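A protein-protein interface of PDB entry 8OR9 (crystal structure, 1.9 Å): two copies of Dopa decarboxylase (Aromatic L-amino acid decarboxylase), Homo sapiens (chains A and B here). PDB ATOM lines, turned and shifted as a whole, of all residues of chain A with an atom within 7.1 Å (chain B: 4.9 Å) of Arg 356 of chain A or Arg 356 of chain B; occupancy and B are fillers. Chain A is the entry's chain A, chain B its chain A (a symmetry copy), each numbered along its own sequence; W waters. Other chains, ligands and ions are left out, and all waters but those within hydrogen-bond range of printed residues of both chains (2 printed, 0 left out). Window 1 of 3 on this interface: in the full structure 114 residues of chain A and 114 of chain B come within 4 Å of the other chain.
OD1 of Asp 92 of chain A lies within salt-bridge range of NH1 of Arg 356 of chain A.
OD1 of Asp 310 of chain A lies within salt-bridge range of NH2 of Arg 356 of chain A (3.0 Å).
The side-chain carboxylate of Asp 92 of chain B is in salt-bridge range of the guanidinium group of Arg 356 of chain B (3.0 Å).
The side-chain carboxylate (OD1) of Asp 310 of chain B is in salt-bridge range of the guanidinium group (NH2) of Arg 356 of chain B.
Phe 309 of chain A touches Arg 356 of chain B, and with the chains exchanged Arg 356 of chain A touches Phe 309 of chain B.
Arg 356 of chain A touches its own counterpart, Arg 356 of chain B.
Positions printed for both chains: 92, 95, 100, 111, 309, 310, 354, 355, 356, 357, 358 and 361.
Of the 12 printed residues of chain B, 2 touch a printed residue of chain A.
Printed residues of chain B that touch a printed residue of chain A: Phe 309 and Arg 356.
Hydrophobic or aromatic side chains of chain B that line the printed part of chain A: Phe 309.
Of the 24 printed residues of chain A, 3 touch a printed residue of chain B.
Hydrophobic or aromatic side chains of chain A within 4 Å of the printed part of chain B: Ile 101 and Phe 309.
Among the printed residues, 4 pairs touch across the chains.
Water W1 lies within hydrogen-bond range of OD2 of Asp 92 of chain A and O of Asp 92 of chain B.
Water W2 lies within hydrogen-bond range of OD2 of Asp 92 of chain B (2.6 Å), O of Asp 92 of chain A (2.8 Å) and N of Gly 96 of chain A (3.5 Å).
Arg 356 of chain A touches just these residues of chain B: Phe 309 (3.9 Å) and Arg 356 (3.1 Å).
Of chain A, only Phe 309 and Arg 356 come within 4 Å of Arg 356 of chain B.
Printed residues of chain A within 4 Å of Phe 309 of chain B: Ile 101 (3.6 Å) and Arg 356 (3.9 Å).
Printed residues of chain B within 4 Å of Phe 309 of chain A: Arg 356.
Asp 310 of chain A touches none of the printed residues of chain B.
Cys 95 of chain B touches none of the printed residues of chain A.
The guanidinium group (NH2) of Arg 356 of chain A sits close to the guanidinium group (NH2) of Arg 356 of chain B (3.1 Å).
Among the printed residues, merely in contact across the chains: Ile 101 of chain A with Phe 309 of chain B (3.6 Å), Phe 309 of chain A with Arg 356 of chain B (3.9 Å) and Arg 356 of chain A with Phe 309 of chain B (3.9 Å).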
ATOM      1  N   ALA A  91     -31.055  29.817  11.790  1.00  0.00           N
ATOM      2  CA  ALA A  91     -29.989  30.643  11.237  1.00  0.00           C
ATOM      3  C   ALA A  91     -29.055  29.821  10.360  1.00  0.00           C
ATOM      4  O   ALA A  91     -28.559  30.314   9.339  1.00  0.00           O
ATOM      5  CB  ALA A  91     -29.215  31.321  12.367  1.00  0.00           C
ATOM      6  N   ASP A  92     -28.809  28.563  10.740  1.00  0.00           N
ATOM      7  CA  ASP A  92     -27.962  27.688   9.934  1.00  0.00           C
ATOM      8  C   ASP A  92     -28.555  27.471   8.547  1.00  0.00           C
ATOM      9  O   ASP A  92     -27.825  27.435   7.549  1.00  0.00           O
ATOM     10  CB  ASP A  92     -27.761  26.352  10.651  1.00  0.00           C
ATOM     11  CG  ASP A  92     -26.302  25.927  10.715  1.00  0.00           C
ATOM     12  OD1 ASP A  92     -25.434  26.650  10.181  1.00  0.00           O
ATOM     13  OD2 ASP A  92     -26.022  24.864  11.308  1.00  0.00           O
ATOM     14  N   CYS A  95     -27.853  30.602   6.762  1.00  0.00           N
ATOM     15  CA  CYS A  95     -26.419  30.687   6.494  1.00  0.00           C
ATOM     16  C   CYS A  95     -26.045  29.908   5.239  1.00  0.00           C
ATOM     17  O   CYS A  95     -25.325  30.414   4.371  1.00  0.00           O
ATOM     18  CB  CYS A  95     -25.631  30.179   7.703  1.00  0.00           C
ATOM     19  SG  CYS A  95     -23.831  30.198   7.491  1.00  0.00           S
ATOM     20  N   GLY A  96     -26.519  28.665   5.129  1.00  0.00           N
ATOM     21  CA  GLY A  96     -26.256  27.878   3.936  1.00  0.00           C
ATOM     22  C   GLY A  96     -26.934  28.409   2.689  1.00  0.00           C
ATOM     23  O   GLY A  96     -26.459  28.152   1.576  1.00  0.00           O
ATOM     24  N   GLY A  99     -24.830  31.421   1.682  1.00  0.00           N
ATOM     25  CA  GLY A  99     -23.741  30.628   1.125  1.00  0.00           C
ATOM     26  C   GLY A  99     -22.512  31.413   0.726  1.00  0.00           C
ATOM     27  O   GLY A  99     -21.867  31.081  -0.277  1.00  0.00           O
ATOM     28  N   CYS A 100     -22.170  32.447   1.486  1.00  0.00           N
ATOM     29  CA  CYS A 100     -20.987  33.243   1.201  1.00  0.00           C
ATOM     30  C   CYS A 100     -19.783  32.694   1.954  1.00  0.00           C
ATOM     31  O   CYS A 100     -19.914  32.074   3.013  1.00  0.00           O
ATOM     32  CB  CYS A 100     -21.209  34.708   1.584  1.00  0.00           C
ATOM     33  SG  CYS A 100     -21.508  34.979   3.353  1.00  0.00           S
ATOM     34  N   ILE A 101     -18.602  32.925   1.392  1.00  0.00           N
ATOM     35  CA  ILE A 101     -17.336  32.579   2.026  1.00  0.00           C
ATOM     36  C   ILE A 101     -16.656  33.897   2.368  1.00  0.00           C
ATOM     37  O   ILE A 101     -15.985  34.502   1.524  1.00  0.00           O
ATOM     38  CB  ILE A 101     -16.456  31.706   1.124  1.00  0.00           C
ATOM     39  CG1 ILE A 101     -17.240  30.486   0.636  1.00  0.00           C
ATOM     40  CG2 ILE A 101     -15.189  31.278   1.859  1.00  0.00           C
ATOM     41  CD1 ILE A 101     -17.416  29.412   1.688  1.00  0.00           C
ATOM     42  N   GLY A 102     -16.830  34.352   3.606  1.00  0.00           N
ATOM     43  CA  GLY A 102     -16.369  35.670   3.994  1.00  0.00           C
ATOM     44  C   GLY A 102     -14.899  35.755   4.343  1.00  0.00           C
ATOM     45  O   GLY A 102     -14.545  36.190   5.443  1.00  0.00           O
ATOM     46  N   PHE A 103     -14.026  35.355   3.413  1.00  0.00           N
ATOM     47  CA  PHE A 103     -12.592  35.522   3.623  1.00  0.00           C
ATOM     48  C   PHE A 103     -12.151  36.974   3.497  1.00  0.00           C
ATOM     49  O   PHE A 103     -11.013  37.294   3.853  1.00  0.00           O
ATOM     50  CB  PHE A 103     -11.799  34.656   2.639  1.00  0.00           C
ATOM     51  CG  PHE A 103     -12.140  34.901   1.193  1.00  0.00           C
ATOM     52  CD1 PHE A 103     -11.575  35.960   0.499  1.00  0.00           C
ATOM     53  CD2 PHE A 103     -13.016  34.063   0.525  1.00  0.00           C
ATOM     54  CE1 PHE A 103     -11.888  36.185  -0.830  1.00  0.00           C
ATOM     55  CE2 PHE A 103     -13.330  34.282  -0.804  1.00  0.00           C
ATOM     56  CZ  PHE A 103     -12.765  35.344  -1.480  1.00  0.00           C
ATOM     57  N   CYS A 111     -21.271  39.458   6.455  1.00  0.00           N
ATOM     58  CA  CYS A 111     -20.702  38.290   7.119  1.00  0.00           C
ATOM     59  C   CYS A 111     -19.655  38.689   8.153  1.00  0.00           C
ATOM     60  O   CYS A 111     -19.531  38.035   9.194  1.00  0.00           O
ATOM     61  CB  CYS A 111     -20.101  37.330   6.089  1.00  0.00           C
ATOM     62  SG  CYS A 111     -19.453  35.789   6.797  1.00  0.00           S
ATOM     63  N   GLU A 115     -20.650  39.757  12.692  1.00  0.00           N
ATOM     64  CA  GLU A 115     -19.818  39.010  13.629  1.00  0.00           C
ATOM     65  C   GLU A 115     -19.192  39.935  14.663  1.00  0.00           C
ATOM     66  O   GLU A 115     -19.195  39.637  15.863  1.00  0.00           O
ATOM     67  CB  GLU A 115     -18.746  38.239  12.860  1.00  0.00           C
ATOM     68  CG  GLU A 115     -17.841  37.389  13.730  1.00  0.00           C
ATOM     69  CD  GLU A 115     -17.149  36.288  12.949  1.00  0.00           C
ATOM     70  OE1 GLU A 115     -17.783  35.709  12.041  1.00  0.00           O
ATOM     71  OE2 GLU A 115     -15.971  36.000  13.249  1.00  0.00           O
ATOM     72  N   ILE A 144     -15.121  35.037  15.882  1.00  0.00           N
ATOM     73  CA  ILE A 144     -15.586  33.661  15.992  1.00  0.00           C
ATOM     74  C   ILE A 144     -14.499  32.735  15.469  1.00  0.00           C
ATOM     75  O   ILE A 144     -13.995  32.912  14.354  1.00  0.00           O
ATOM     76  CB  ILE A 144     -16.899  33.456  15.220  1.00  0.00           C
ATOM     77  CG1 ILE A 144     -18.006  34.349  15.780  1.00  0.00           C
ATOM     78  CG2 ILE A 144     -17.321  31.993  15.278  1.00  0.00           C
ATOM     79  CD1 ILE A 144     -19.292  34.256  14.994  1.00  0.00           C
ATOM     80  N   ASN A 308     -25.375  26.418  17.947  1.00  0.00           N
ATOM     81  CA  ASN A 308     -24.910  25.145  17.398  1.00  0.00           C
ATOM     82  C   ASN A 308     -23.488  25.244  16.847  1.00  0.00           C
ATOM     83  O   ASN A 308     -23.109  26.246  16.235  1.00  0.00           O
ATOM     84  CB  ASN A 308     -25.857  24.672  16.291  1.00  0.00           C
ATOM     85  CG  ASN A 308     -27.263  24.396  16.796  1.00  0.00           C
ATOM     86  OD1 ASN A 308     -27.610  24.741  17.924  1.00  0.00           O
ATOM     87  ND2 ASN A 308     -28.080  23.772  15.957  1.00  0.00           N
ATOM     88  N   PHE A 309     -22.704  24.188  17.087  1.00  0.00           N
ATOM     89  CA  PHE A 309     -21.365  24.050  16.515  1.00  0.00           C
ATOM     90  C   PHE A 309     -21.404  24.259  15.006  1.00  0.00           C
ATOM     91  O   PHE A 309     -22.286  23.733  14.322  1.00  0.00           O
ATOM     92  CB  PHE A 309     -20.819  22.652  16.850  1.00  0.00           C
ATOM     93  CG  PHE A 309     -19.371  22.438  16.481  1.00  0.00           C
ATOM     94  CD1 PHE A 309     -19.013  22.015  15.209  1.00  0.00           C
ATOM     95  CD2 PHE A 309     -18.370  22.625  17.422  1.00  0.00           C
ATOM     96  CE1 PHE A 309     -17.683  21.807  14.877  1.00  0.00           C
ATOM     97  CE2 PHE A 309     -17.040  22.418  17.096  1.00  0.00           C
ATOM     98  CZ  PHE A 309     -16.696  22.009  15.821  1.00  0.00           C
ATOM     99  N   ASP A 310     -20.445  25.021  14.476  1.00  0.00           N
ATOM    100  CA  ASP A 310     -19.321  25.580  15.228  1.00  0.00           C
ATOM    101  C   ASP A 310     -19.513  27.058  15.575  1.00  0.00           C
ATOM    102  O   ASP A 310     -20.012  27.841  14.771  1.00  0.00           O
ATOM    103  CB  ASP A 310     -18.021  25.410  14.431  1.00  0.00           C
ATOM    104  CG  ASP A 310     -18.149  25.897  12.994  1.00  0.00           C
ATOM    105  OD1 ASP A 310     -19.229  25.708  12.395  1.00  0.00           O
ATOM    106  OD2 ASP A 310     -17.173  26.472  12.463  1.00  0.00           O
ATOM    107  N   CYS A 311     -19.101  27.414  16.796  1.00  0.00           N
ATOM    108  CA  CYS A 311     -19.113  28.803  17.264  1.00  0.00           C
ATOM    109  C   CYS A 311     -18.289  28.876  18.550  1.00  0.00           C
ATOM    110  O   CYS A 311     -18.789  28.531  19.624  1.00  0.00           O
ATOM    111  CB  CYS A 311     -20.527  29.310  17.500  1.00  0.00           C
ATOM    112  SG  CYS A 311     -20.607  31.030  18.103  1.00  0.00           S
ATOM    113  N   GLY A 354     -11.055  30.749   4.549  1.00  0.00           N
ATOM    114  CA  GLY A 354     -12.485  30.806   4.359  1.00  0.00           C
ATOM    115  C   GLY A 354     -13.256  30.654   5.658  1.00  0.00           C
ATOM    116  O   GLY A 354     -12.760  30.127   6.655  1.00  0.00           O
ATOM    117  N   ARG A 355     -14.496  31.134   5.634  1.00  0.00           N
ATOM    118  CA  ARG A 355     -15.388  31.091   6.786  1.00  0.00           C
ATOM    119  C   ARG A 355     -16.803  31.375   6.306  1.00  0.00           C
ATOM    120  O   ARG A 355     -17.000  32.073   5.308  1.00  0.00           O
ATOM    121  CB  ARG A 355     -14.970  32.107   7.858  1.00  0.00           C
ATOM    122  CG  ARG A 355     -14.977  33.551   7.379  1.00  0.00           C
ATOM    123  CD  ARG A 355     -13.910  34.378   8.083  1.00  0.00           C
ATOM    124  NE  ARG A 355     -13.856  34.089   9.513  1.00  0.00           N
ATOM    125  CZ  ARG A 355     -14.667  34.631  10.416  1.00  0.00           C
ATOM    126  NH1 ARG A 355     -15.598  35.496  10.036  1.00  0.00           N
ATOM    127  NH2 ARG A 355     -14.548  34.307  11.699  1.00  0.00           N
ATOM    128  N   ARG A 356     -17.781  30.824   7.019  1.00  0.00           N
ATOM    129  CA  ARG A 356     -19.182  31.016   6.678  1.00  0.00           C
ATOM    130  C   ARG A 356     -19.840  31.969   7.675  1.00  0.00           C
ATOM    131  O   ARG A 356     -19.235  32.400   8.660  1.00  0.00           O
ATOM    132  CB  ARG A 356     -19.916  29.672   6.606  1.00  0.00           C
ATOM    133  CG  ARG A 356     -19.837  28.818   7.856  1.00  0.00           C
ATOM    134  CD  ARG A 356     -20.345  27.410   7.573  1.00  0.00           C
ATOM    135  NE  ARG A 356     -20.429  26.602   8.786  1.00  0.00           N
ATOM    136  CZ  ARG A 356     -21.571  26.226   9.354  1.00  0.00           C
ATOM    137  NH1 ARG A 356     -22.731  26.578   8.818  1.00  0.00           N
ATOM    138  NH2 ARG A 356     -21.552  25.495  10.461  1.00  0.00           N
ATOM    139  N   PHE A 357     -21.104  32.293   7.395  1.00  0.00           N
ATOM    140  CA  PHE A 357     -21.852  33.333   8.106  1.00  0.00           C
ATOM    141  C   PHE A 357     -22.317  32.838   9.480  1.00  0.00           C
ATOM    142  O   PHE A 357     -23.508  32.789   9.789  1.00  0.00           O
ATOM    143  CB  PHE A 357     -23.032  33.772   7.246  1.00  0.00           C
ATOM    144  CG  PHE A 357     -23.480  35.190   7.479  1.00  0.00           C
ATOM    145  CD1 PHE A 357     -23.203  35.847   8.666  1.00  0.00           C
ATOM    146  CD2 PHE A 357     -24.193  35.861   6.499  1.00  0.00           C
ATOM    147  CE1 PHE A 357     -23.626  37.150   8.869  1.00  0.00           C
ATOM    148  CE2 PHE A 357     -24.618  37.165   6.694  1.00  0.00           C
ATOM    149  CZ  PHE A 357     -24.334  37.809   7.881  1.00  0.00           C
ATOM    150  N   ARG A 358     -21.338  32.493  10.322  1.00  0.00           N
ATOM    151  CA  ARG A 358     -21.636  31.890  11.618  1.00  0.00           C
ATOM    152  C   ARG A 358     -22.293  32.860  12.592  1.00  0.00           C
ATOM    153  O   ARG A 358     -22.976  32.412  13.520  1.00  0.00           O
ATOM    154  CB  ARG A 358     -20.358  31.323  12.240  1.00  0.00           C
ATOM    155  CG  ARG A 358     -19.821  30.091  11.526  1.00  0.00           C
ATOM    156  CD  ARG A 358     -18.537  29.584  12.169  1.00  0.00           C
ATOM    157  NE  ARG A 358     -17.422  30.501  11.958  1.00  0.00           N
ATOM    158  CZ  ARG A 358     -16.143  30.140  11.966  1.00  0.00           C
ATOM    159  NH1 ARG A 358     -15.809  28.874  12.181  1.00  0.00           N
ATOM    160  NH2 ARG A 358     -15.199  31.048  11.765  1.00  0.00           N
ATOM    161  N   SER A 359     -22.109  34.169  12.411  1.00  0.00           N
ATOM    162  CA  SER A 359     -22.689  35.130  13.344  1.00  0.00           C
ATOM    163  C   SER A 359     -24.211  35.148  13.292  1.00  0.00           C
ATOM    164  O   SER A 359     -24.842  35.627  14.241  1.00  0.00           O
ATOM    165  CB  SER A 359     -22.152  36.532  13.066  1.00  0.00           C
ATOM    166  OG  SER A 359     -22.272  36.862  11.695  1.00  0.00           O
ATOM    167  N   LEU A 360     -24.811  34.651  12.207  1.00  0.00           N
ATOM    168  CA  LEU A 360     -26.266  34.549  12.151  1.00  0.00           C
ATOM    169  C   LEU A 360     -26.797  33.664  13.274  1.00  0.00           C
ATOM    170  O   LEU A 360     -27.874  33.928  13.823  1.00  0.00           O
ATOM    171  CB  LEU A 360     -26.701  34.005  10.790  1.00  0.00           C
ATOM    172  CG  LEU A 360     -26.702  34.978   9.611  1.00  0.00           C
ATOM    173  CD1 LEU A 360     -27.013  34.235   8.320  1.00  0.00           C
ATOM    174  CD2 LEU A 360     -27.699  36.106   9.839  1.00  0.00           C
ATOM    175  N   LYS A 361     -26.053  32.614  13.632  1.00  0.00           N
ATOM    176  CA  LYS A 361     -26.485  31.740  14.719  1.00  0.00           C
ATOM    177  C   LYS A 361     -26.492  32.478  16.052  1.00  0.00           C
ATOM    178  O   LYS A 361     -27.433  32.339  16.842  1.00  0.00           O
ATOM    179  CB  LYS A 361     -25.586  30.505  14.793  1.00  0.00           C
ATOM    180  CG  LYS A 361     -25.731  29.557  13.610  1.00  0.00           C
ATOM    181  CD  LYS A 361     -24.909  28.296  13.810  1.00  0.00           C
ATOM    182  CE  LYS A 361     -23.415  28.596  13.799  1.00  0.00           C
ATOM    183  NZ  LYS A 361     -22.612  27.338  13.925  1.00  0.00           N
ATOM    184  N   ASP B  92     -27.509  19.281   5.970  1.00  0.00           N
ATOM    185  CA  ASP B  92     -27.072  20.221   6.999  1.00  0.00           C
ATOM    186  C   ASP B  92     -28.118  20.355   8.102  1.00  0.00           C
ATOM    187  O   ASP B  92     -27.773  20.445   9.286  1.00  0.00           O
ATOM    188  CB  ASP B  92     -26.775  21.583   6.368  1.00  0.00           C
ATOM    189  CG  ASP B  92     -25.429  22.149   6.793  1.00  0.00           C
ATOM    190  OD1 ASP B  92     -24.724  21.506   7.600  1.00  0.00           O
ATOM    191  OD2 ASP B  92     -25.071  23.245   6.311  1.00  0.00           O
ATOM    192  N   CYS B  95     -27.753  17.278  10.071  1.00  0.00           N
ATOM    193  CA  CYS B  95     -26.492  17.329  10.808  1.00  0.00           C
ATOM    194  C   CYS B  95     -26.640  18.121  12.102  1.00  0.00           C
ATOM    195  O   CYS B  95     -26.208  17.673  13.171  1.00  0.00           O
ATOM    196  CB  CYS B  95     -25.396  17.933   9.926  1.00  0.00           C
ATOM    197  SG  CYS B  95     -23.781  18.088  10.732  1.00  0.00           S
ATOM    198  N   CYS B 100     -24.025  15.910  16.984  1.00  0.00           N
ATOM    199  CA  CYS B 100     -22.935  15.229  17.664  1.00  0.00           C
ATOM    200  C   CYS B 100     -21.607  15.907  17.351  1.00  0.00           C
ATOM    201  O   CYS B 100     -21.435  16.528  16.299  1.00  0.00           O
ATOM    202  CB  CYS B 100     -22.870  13.757  17.254  1.00  0.00           C
ATOM    203  SG  CYS B 100     -22.528  13.487  15.493  1.00  0.00           S
ATOM    204  N   CYS B 111     -20.822   9.107  12.728  1.00  0.00           N
ATOM    205  CA  CYS B 111     -20.181  10.336  12.274  1.00  0.00           C
ATOM    206  C   CYS B 111     -18.813  10.060  11.660  1.00  0.00           C
ATOM    207  O   CYS B 111     -18.411  10.740  10.711  1.00  0.00           O
ATOM    208  CB  CYS B 111     -20.059  11.333  13.430  1.00  0.00           C
ATOM    209  SG  CYS B 111     -19.365  12.942  12.955  1.00  0.00           S
ATOM    210  N   PHE B 309     -20.085  24.341   1.975  1.00  0.00           N
ATOM    211  CA  PHE B 309     -19.037  24.600   2.962  1.00  0.00           C
ATOM    212  C   PHE B 309     -19.561  24.363   4.373  1.00  0.00           C
ATOM    213  O   PHE B 309     -20.669  24.788   4.711  1.00  0.00           O
ATOM    214  CB  PHE B 309     -18.550  26.051   2.807  1.00  0.00           C
ATOM    215  CG  PHE B 309     -17.339  26.401   3.637  1.00  0.00           C
ATOM    216  CD1 PHE B 309     -17.474  26.834   4.949  1.00  0.00           C
ATOM    217  CD2 PHE B 309     -16.066  26.328   3.091  1.00  0.00           C
ATOM    218  CE1 PHE B 309     -16.360  27.166   5.705  1.00  0.00           C
ATOM    219  CE2 PHE B 309     -14.951  26.659   3.843  1.00  0.00           C
ATOM    220  CZ  PHE B 309     -15.098  27.078   5.152  1.00  0.00           C
ATOM    221  N   ASP B 310     -18.766  23.690   5.208  1.00  0.00           N
ATOM    222  CA  ASP B 310     -17.407  23.257   4.888  1.00  0.00           C
ATOM    223  C   ASP B 310     -17.324  21.774   4.521  1.00  0.00           C
ATOM    224  O   ASP B 310     -17.985  20.932   5.124  1.00  0.00           O
ATOM    225  CB  ASP B 310     -16.473  23.540   6.072  1.00  0.00           C
ATOM    226  CG  ASP B 310     -17.029  23.019   7.390  1.00  0.00           C
ATOM    227  OD1 ASP B 310     -18.261  23.090   7.588  1.00  0.00           O
ATOM    228  OD2 ASP B 310     -16.237  22.533   8.229  1.00  0.00           O
ATOM    229  N   GLY B 354     -12.751  18.743  17.813  1.00  0.00           N
ATOM    230  CA  GLY B 354     -14.150  18.543  17.510  1.00  0.00           C
ATOM    231  C   GLY B 354     -14.449  18.641  16.026  1.00  0.00           C
ATOM    232  O   GLY B 354     -13.701  19.231  15.245  1.00  0.00           O
ATOM    233  N   ARG B 355     -15.572  18.041  15.639  1.00  0.00           N
ATOM    234  CA  ARG B 355     -16.023  18.015  14.254  1.00  0.00           C
ATOM    235  C   ARG B 355     -17.481  17.586  14.234  1.00  0.00           C
ATOM    236  O   ARG B 355     -17.934  16.855  15.120  1.00  0.00           O
ATOM    237  CB  ARG B 355     -15.171  17.064  13.403  1.00  0.00           C
ATOM    238  CG  ARG B 355     -15.197  15.618  13.876  1.00  0.00           C
ATOM    239  CD  ARG B 355     -13.880  14.912  13.586  1.00  0.00           C
ATOM    240  NE  ARG B 355     -13.376  15.230  12.252  1.00  0.00           N
ATOM    241  CZ  ARG B 355     -13.778  14.626  11.139  1.00  0.00           C
ATOM    242  NH1 ARG B 355     -14.694  13.667  11.198  1.00  0.00           N
ATOM    243  NH2 ARG B 355     -13.267  14.982   9.966  1.00  0.00           N
ATOM    244  N   ARG B 356     -18.212  18.050  13.225  1.00  0.00           N
ATOM    245  CA  ARG B 356     -19.620  17.716  13.076  1.00  0.00           C
ATOM    246  C   ARG B 356     -19.808  16.720  11.933  1.00  0.00           C
ATOM    247  O   ARG B 356     -18.867  16.367  11.217  1.00  0.00           O
ATOM    248  CB  ARG B 356     -20.464  18.980  12.875  1.00  0.00           C
ATOM    249  CG  ARG B 356     -20.054  19.858  11.710  1.00  0.00           C
ATOM    250  CD  ARG B 356     -20.762  21.205  11.781  1.00  0.00           C
ATOM    251  NE  ARG B 356     -20.512  22.021  10.597  1.00  0.00           N
ATOM    252  CZ  ARG B 356     -21.426  22.293   9.672  1.00  0.00           C
ATOM    253  NH1 ARG B 356     -22.658  21.820   9.792  1.00  0.00           N
ATOM    254  NH2 ARG B 356     -21.108  23.041   8.624  1.00  0.00           N
ATOM    255  N   PHE B 357     -21.053  16.269  11.776  1.00  0.00           N
ATOM    256  CA  PHE B 357     -21.412  15.173  10.874  1.00  0.00           C
ATOM    257  C   PHE B 357     -21.434  15.643   9.415  1.00  0.00           C
ATOM    258  O   PHE B 357     -22.450  15.580   8.722  1.00  0.00           O
ATOM    259  CB  PHE B 357     -22.764  14.606  11.293  1.00  0.00           C
ATOM    260  CG  PHE B 357     -22.966  13.155  10.947  1.00  0.00           C
ATOM    261  CD1 PHE B 357     -22.242  12.548   9.934  1.00  0.00           C
ATOM    262  CD2 PHE B 357     -23.898  12.400  11.642  1.00  0.00           C
ATOM    263  CE1 PHE B 357     -22.443  11.214   9.623  1.00  0.00           C
ATOM    264  CE2 PHE B 357     -24.102  11.064  11.337  1.00  0.00           C
ATOM    265  CZ  PHE B 357     -23.373  10.472  10.326  1.00  0.00           C
ATOM    266  N   ARG B 358     -20.268  16.097   8.945  1.00  0.00           N
ATOM    267  CA  ARG B 358     -20.170  16.690   7.615  1.00  0.00           C
ATOM    268  C   ARG B 358     -20.362  15.676   6.494  1.00  0.00           C
ATOM    269  O   ARG B 358     -20.732  16.071   5.382  1.00  0.00           O
ATOM    270  CB  ARG B 358     -18.819  17.390   7.450  1.00  0.00           C
ATOM    271  CG  ARG B 358     -18.677  18.656   8.281  1.00  0.00           C
ATOM    272  CD  ARG B 358     -17.308  19.297   8.100  1.00  0.00           C
ATOM    273  NE  ARG B 358     -16.245  18.491   8.689  1.00  0.00           N
ATOM    274  CZ  ARG B 358     -15.080  18.976   9.106  1.00  0.00           C
ATOM    275  NH1 ARG B 358     -14.818  20.272   8.995  1.00  0.00           N
ATOM    276  NH2 ARG B 358     -14.174  18.162   9.629  1.00  0.00           N
ATOM    277  N   LYS B 361     -23.557  15.570   4.244  1.00  0.00           N
ATOM    278  CA  LYS B 361     -23.681  16.416   3.061  1.00  0.00           C
ATOM    279  C   LYS B 361     -23.167  15.703   1.816  1.00  0.00           C
ATOM    280  O   LYS B 361     -23.796  15.762   0.753  1.00  0.00           O
ATOM    281  CB  LYS B 361     -22.936  17.734   3.273  1.00  0.00           C
ATOM    282  CG  LYS B 361     -23.563  18.643   4.322  1.00  0.00           C
ATOM    283  CD  LYS B 361     -22.849  19.982   4.388  1.00  0.00           C
ATOM    284  CE  LYS B 361     -21.424  19.830   4.906  1.00  0.00           C
ATOM    285  NZ  LYS B 361     -20.754  21.162   5.037  1.00  0.00           N
HETATM  286  O   HOH W   1     -26.287  22.337  10.653  1.00  0.00           O
HETATM  287  O   HOH W   2     -25.788  25.722   6.795  1.00  0.00           O
